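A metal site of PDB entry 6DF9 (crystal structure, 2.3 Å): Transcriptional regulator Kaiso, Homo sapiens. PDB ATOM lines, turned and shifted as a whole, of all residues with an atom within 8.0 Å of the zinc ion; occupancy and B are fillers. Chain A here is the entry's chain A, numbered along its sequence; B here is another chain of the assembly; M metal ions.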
ATOM      1  N   ASP A  12     -30.723 -20.520  27.127  1.00  0.00           N
ATOM      2  CA  ASP A  12     -29.463 -21.028  27.681  1.00  0.00           C
ATOM      3  C   ASP A  12     -28.356 -21.289  26.636  1.00  0.00           C
ATOM      4  O   ASP A  12     -27.167 -21.014  26.874  1.00  0.00           O
ATOM      5  CB  ASP A  12     -29.736 -22.311  28.449  1.00  0.00           C
ATOM      6  CG  ASP A  12     -28.480 -23.124  28.670  1.00  0.00           C
ATOM      7  OD1 ASP A  12     -27.500 -22.574  29.218  1.00  0.00           O
ATOM      8  OD2 ASP A  12     -28.467 -24.310  28.266  1.00  0.00           O
ATOM      9  N   ILE A  25     -23.858 -24.234  21.476  1.00  0.00           N
ATOM     10  CA  ILE A  25     -23.302 -22.888  21.559  1.00  0.00           C
ATOM     11  C   ILE A  25     -23.846 -22.106  22.747  1.00  0.00           C
ATOM     12  O   ILE A  25     -25.054 -21.948  22.904  1.00  0.00           O
ATOM     13  CB  ILE A  25     -23.581 -22.046  20.303  1.00  0.00           C
ATOM     14  CG1 ILE A  25     -23.476 -22.895  19.029  1.00  0.00           C
ATOM     15  CG2 ILE A  25     -22.664 -20.838  20.275  1.00  0.00           C
ATOM     16  CD1 ILE A  25     -22.127 -23.580  18.842  1.00  0.00           C
ATOM     17  N   CYS A  26     -22.929 -21.620  23.577  1.00  0.00           N
ATOM     18  CA  CYS A  26     -23.279 -20.746  24.684  1.00  0.00           C
ATOM     19  C   CYS A  26     -23.875 -19.444  24.188  1.00  0.00           C
ATOM     20  O   CYS A  26     -23.262 -18.747  23.386  1.00  0.00           O
ATOM     21  CB  CYS A  26     -22.047 -20.475  25.538  1.00  0.00           C
ATOM     22  SG  CYS A  26     -22.288 -19.253  26.767  1.00  0.00           S
ATOM     23  N   ILE A  27     -25.068 -19.119  24.689  1.00  0.00           N
ATOM     24  CA  ILE A  27     -25.774 -17.903  24.296  1.00  0.00           C
ATOM     25  C   ILE A  27     -24.932 -16.640  24.460  1.00  0.00           C
ATOM     26  O   ILE A  27     -24.954 -15.748  23.607  1.00  0.00           O
ATOM     27  CB  ILE A  27     -27.092 -17.730  25.110  1.00  0.00           C
ATOM     28  CG1 ILE A  27     -28.220 -18.562  24.497  1.00  0.00           C
ATOM     29  CG2 ILE A  27     -27.519 -16.273  25.140  1.00  0.00           C
ATOM     30  CD1 ILE A  27     -29.579 -18.309  25.110  1.00  0.00           C
ATOM     31  N   VAL A  28     -24.192 -16.576  25.564  1.00  0.00           N
ATOM     32  CA  VAL A  28     -23.518 -15.349  25.949  1.00  0.00           C
ATOM     33  C   VAL A  28     -22.224 -15.107  25.173  1.00  0.00           C
ATOM     34  O   VAL A  28     -22.051 -14.042  24.577  1.00  0.00           O
ATOM     35  CB  VAL A  28     -23.188 -15.337  27.464  1.00  0.00           C
ATOM     36  CG1 VAL A  28     -22.326 -14.141  27.810  1.00  0.00           C
ATOM     37  CG2 VAL A  28     -24.470 -15.306  28.291  1.00  0.00           C
ATOM     38  N   CYS A  29     -21.315 -16.073  25.177  1.00  0.00           N
ATOM     39  CA  CYS A  29     -20.002 -15.838  24.591  1.00  0.00           C
ATOM     40  C   CYS A  29     -19.801 -16.574  23.281  1.00  0.00           C
ATOM     41  O   CYS A  29     -18.787 -16.378  22.615  1.00  0.00           O
ATOM     42  CB  CYS A  29     -18.892 -16.206  25.580  1.00  0.00           C
ATOM     43  SG  CYS A  29     -18.790 -17.943  26.044  1.00  0.00           S
ATOM     44  N   LYS A  30     -20.769 -17.413  22.928  1.00  0.00           N
ATOM     45  CA  LYS A  30     -20.752 -18.167  21.669  1.00  0.00           C
ATOM     46  C   LYS A  30     -19.635 -19.232  21.566  1.00  0.00           C
ATOM     47  O   LYS A  30     -19.332 -19.691  20.472  1.00  0.00           O
ATOM     48  CB  LYS A  30     -20.639 -17.204  20.473  1.00  0.00           C
ATOM     49  CG  LYS A  30     -21.965 -16.957  19.755  1.00  0.00           C
ATOM     50  CD  LYS A  30     -21.836 -15.978  18.584  1.00  0.00           C
ATOM     51  CE  LYS A  30     -21.544 -16.691  17.267  1.00  0.00           C
ATOM     52  NZ  LYS A  30     -20.970 -15.787  16.230  1.00  0.00           N
ATOM     53  N   ARG A  31     -19.049 -19.638  22.705  1.00  0.00           N
ATOM     54  CA  ARG A  31     -18.129 -20.792  22.705  1.00  0.00           C
ATOM     55  C   ARG A  31     -18.893 -22.033  22.300  1.00  0.00           C
ATOM     56  O   ARG A  31     -20.113 -22.104  22.485  1.00  0.00           O
ATOM     57  CB  ARG A  31     -17.498 -21.014  24.082  1.00  0.00           C
ATOM     58  CG  ARG A  31     -16.358 -20.075  24.400  1.00  0.00           C
ATOM     59  CD  ARG A  31     -15.879 -20.237  25.861  1.00  0.00           C
ATOM     60  NE  ARG A  31     -14.889 -19.221  26.205  1.00  0.00           N
ATOM     61  CZ  ARG A  31     -13.578 -19.403  26.131  1.00  0.00           C
ATOM     62  NH1 ARG A  31     -13.069 -20.574  25.761  1.00  0.00           N
ATOM     63  NH2 ARG A  31     -12.767 -18.404  26.454  1.00  0.00           N
ATOM     64  N   SER A  32     -18.199 -23.021  21.737  1.00  0.00           N
ATOM     65  CA  SER A  32     -18.905 -24.201  21.236  1.00  0.00           C
ATOM     66  C   SER A  32     -18.441 -25.454  21.969  1.00  0.00           C
ATOM     67  O   SER A  32     -17.270 -25.601  22.298  1.00  0.00           O
ATOM     68  CB  SER A  32     -18.738 -24.371  19.723  1.00  0.00           C
ATOM     69  OG  SER A  32     -17.447 -24.863  19.398  1.00  0.00           O
ATOM     70  N   TYR A  33     -19.384 -26.347  22.221  1.00  0.00           N
ATOM     71  CA  TYR A  33     -19.074 -27.544  22.987  1.00  0.00           C
ATOM     72  C   TYR A  33     -19.608 -28.794  22.307  1.00  0.00           C
ATOM     73  O   TYR A  33     -20.715 -28.792  21.772  1.00  0.00           O
ATOM     74  CB  TYR A  33     -19.638 -27.424  24.392  1.00  0.00           C
ATOM     75  CG  TYR A  33     -19.023 -26.267  25.151  1.00  0.00           C
ATOM     76  CD1 TYR A  33     -19.565 -24.987  25.062  1.00  0.00           C
ATOM     77  CD2 TYR A  33     -17.879 -26.451  25.921  1.00  0.00           C
ATOM     78  CE1 TYR A  33     -18.995 -23.928  25.741  1.00  0.00           C
ATOM     79  CE2 TYR A  33     -17.291 -25.404  26.604  1.00  0.00           C
ATOM     80  CZ  TYR A  33     -17.855 -24.145  26.511  1.00  0.00           C
ATOM     81  OH  TYR A  33     -17.270 -23.097  27.180  1.00  0.00           O
ATOM     82  N   LEU A  39     -21.193 -27.418  28.367  1.00  0.00           N
ATOM     83  CA  LEU A  39     -21.795 -26.108  28.166  1.00  0.00           C
ATOM     84  C   LEU A  39     -22.376 -25.624  29.500  1.00  0.00           C
ATOM     85  O   LEU A  39     -22.120 -24.493  29.923  1.00  0.00           O
ATOM     86  CB  LEU A  39     -22.877 -26.187  27.082  1.00  0.00           C
ATOM     87  CG  LEU A  39     -23.716 -24.970  26.661  1.00  0.00           C
ATOM     88  CD1 LEU A  39     -24.860 -24.717  27.626  1.00  0.00           C
ATOM     89  CD2 LEU A  39     -22.860 -23.734  26.521  1.00  0.00           C
ATOM     90  N   HIS A  42     -19.566 -24.838  32.008  1.00  0.00           N
ATOM     91  CA  HIS A  42     -19.005 -23.552  31.609  1.00  0.00           C
ATOM     92  C   HIS A  42     -19.916 -22.354  31.894  1.00  0.00           C
ATOM     93  O   HIS A  42     -19.437 -21.250  32.173  1.00  0.00           O
ATOM     94  CB  HIS A  42     -18.675 -23.575  30.121  1.00  0.00           C
ATOM     95  CG  HIS A  42     -18.784 -22.236  29.467  1.00  0.00           C
ATOM     96  ND1 HIS A  42     -17.752 -21.331  29.437  1.00  0.00           N
ATOM     97  CD2 HIS A  42     -19.813 -21.650  28.797  1.00  0.00           C
ATOM     98  CE1 HIS A  42     -18.127 -20.249  28.788  1.00  0.00           C
ATOM     99  NE2 HIS A  42     -19.380 -20.413  28.397  1.00  0.00           N
ATOM    100  N   PHE A  43     -21.221 -22.562  31.820  1.00  0.00           N
ATOM    101  CA  PHE A  43     -22.137 -21.421  31.841  1.00  0.00           C
ATOM    102  C   PHE A  43     -22.249 -20.819  33.242  1.00  0.00           C
ATOM    103  O   PHE A  43     -22.738 -19.704  33.400  1.00  0.00           O
ATOM    104  CB  PHE A  43     -23.515 -21.828  31.317  1.00  0.00           C
ATOM    105  CG  PHE A  43     -24.417 -20.659  30.970  1.00  0.00           C
ATOM    106  CD1 PHE A  43     -24.385 -20.094  29.703  1.00  0.00           C
ATOM    107  CD2 PHE A  43     -25.298 -20.137  31.909  1.00  0.00           C
ATOM    108  CE1 PHE A  43     -25.223 -19.026  29.366  1.00  0.00           C
ATOM    109  CE2 PHE A  43     -26.146 -19.061  31.589  1.00  0.00           C
ATOM    110  CZ  PHE A  43     -26.102 -18.504  30.320  1.00  0.00           C
ATOM    111  N   ASN A  44     -21.762 -21.544  34.250  1.00  0.00           N
ATOM    112  CA  ASN A  44     -21.821 -21.005  35.599  1.00  0.00           C
ATOM    113  C   ASN A  44     -20.980 -19.748  35.691  1.00  0.00           C
ATOM    114  O   ASN A  44     -21.307 -18.806  36.415  1.00  0.00           O
ATOM    115  CB  ASN A  44     -21.377 -22.023  36.646  1.00  0.00           C
ATOM    116  CG  ASN A  44     -22.019 -21.774  37.994  1.00  0.00           C
ATOM    117  OD1 ASN A  44     -23.224 -21.504  38.088  1.00  0.00           O
ATOM    118  ND2 ASN A  44     -21.219 -21.813  39.045  1.00  0.00           N
ATOM    119  N   ILE A  45     -19.878 -19.737  34.951  1.00  0.00           N
ATOM    120  CA  ILE A  45     -19.039 -18.550  34.799  1.00  0.00           C
ATOM    121  C   ILE A  45     -19.844 -17.285  34.488  1.00  0.00           C
ATOM    122  O   ILE A  45     -19.557 -16.212  35.019  1.00  0.00           O
ATOM    123  CB  ILE A  45     -18.005 -18.779  33.709  1.00  0.00           C
ATOM    124  CG1 ILE A  45     -17.085 -19.956  34.095  1.00  0.00           C
ATOM    125  CG2 ILE A  45     -17.205 -17.506  33.442  1.00  0.00           C
ATOM    126  CD1 ILE A  45     -16.155 -20.396  32.970  1.00  0.00           C
ATOM    127  N   HIS A  46     -20.867 -17.415  33.651  1.00  0.00           N
ATOM    128  CA  HIS A  46     -21.729 -16.271  33.326  1.00  0.00           C
ATOM    129  C   HIS A  46     -22.786 -16.017  34.391  1.00  0.00           C
ATOM    130  O   HIS A  46     -23.035 -14.871  34.775  1.00  0.00           O
ATOM    131  CB  HIS A  46     -22.423 -16.485  31.983  1.00  0.00           C
ATOM    132  CG  HIS A  46     -21.480 -16.683  30.836  1.00  0.00           C
ATOM    133  ND1 HIS A  46     -20.406 -15.860  30.620  1.00  0.00           N
ATOM    134  CD2 HIS A  46     -21.459 -17.618  29.854  1.00  0.00           C
ATOM    135  CE1 HIS A  46     -19.757 -16.269  29.541  1.00  0.00           C
ATOM    136  NE2 HIS A  46     -20.376 -17.324  29.056  1.00  0.00           N
ATOM    137  P    DT B   8     -13.841 -24.311  27.046  1.00  0.00           P
ATOM    138  OP1  DT B   8     -13.854 -23.522  25.797  1.00  0.00           O
ATOM    139  OP2  DT B   8     -14.702 -23.926  28.189  1.00  0.00           O
ATOM    140  O5'  DT B   8     -14.072 -25.865  26.765  1.00  0.00           O
ATOM    141  C5'  DT B   8     -13.277 -26.552  25.766  1.00  0.00           C
ATOM    142  C4'  DT B   8     -13.338 -28.049  25.995  1.00  0.00           C
ATOM    143  O4'  DT B   8     -12.480 -28.419  27.125  1.00  0.00           O
ATOM    144  C3'  DT B   8     -14.727 -28.630  26.338  1.00  0.00           C
ATOM    145  O3'  DT B   8     -14.849 -29.914  25.740  1.00  0.00           O
ATOM    146  C2'  DT B   8     -14.631 -28.763  27.861  1.00  0.00           C
ATOM    147  C1'  DT B   8     -13.205 -29.279  27.964  1.00  0.00           C
ATOM    148  N1   DT B   8     -12.580 -29.247  29.317  1.00  0.00           N
ATOM    149  C2   DT B   8     -11.521 -30.095  29.577  1.00  0.00           C
ATOM    150  O2   DT B   8     -11.096 -30.894  28.767  1.00  0.00           O
ATOM    151  N3   DT B   8     -10.986 -29.990  30.831  1.00  0.00           N
ATOM    152  C4   DT B   8     -11.387 -29.140  31.831  1.00  0.00           C
ATOM    153  O4   DT B   8     -10.837 -29.130  32.938  1.00  0.00           O
ATOM    154  C5   DT B   8     -12.492 -28.268  31.507  1.00  0.00           C
ATOM    155  C7   DT B   8     -12.991 -27.303  32.547  1.00  0.00           C
ATOM    156  C6   DT B   8     -13.037 -28.353  30.277  1.00  0.00           C
HETATM  157 ZN    ZN M   1     -20.188 -18.667  27.590  1.00  0.00          ZN
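The side-chain hydroxyl (OH) of Tyr 33 lies close to a ring nitrogen (ND1) of His 42 (2.9 Å). The side-chain sulfur (SG) of Cys 29 sits close to the backbone NH (N) of Arg 31 (3.8 Å). N of Val 28 sits close to SG of Cys 26, at 3.5 Å. The backbone carbonyl oxygen of Arg 31 is in hydrogen-bond range of the backbone NH of Cys 26, 3.1 Å away.
Within 4 Å of the zinc ion: Cys 26, Cys 29, His 42 and His 46.
The zinc ion is bound by a ring nitrogen (NE2) of His 46 (2.0 Å), a ring nitrogen (NE2) of His 42 (2.1 Å), the side-chain sulfur of Cys 29 (2.2 Å) and the side-chain sulfur of Cys 26 (2.3 Å). The zinc ion has four donor atoms within binding distance.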
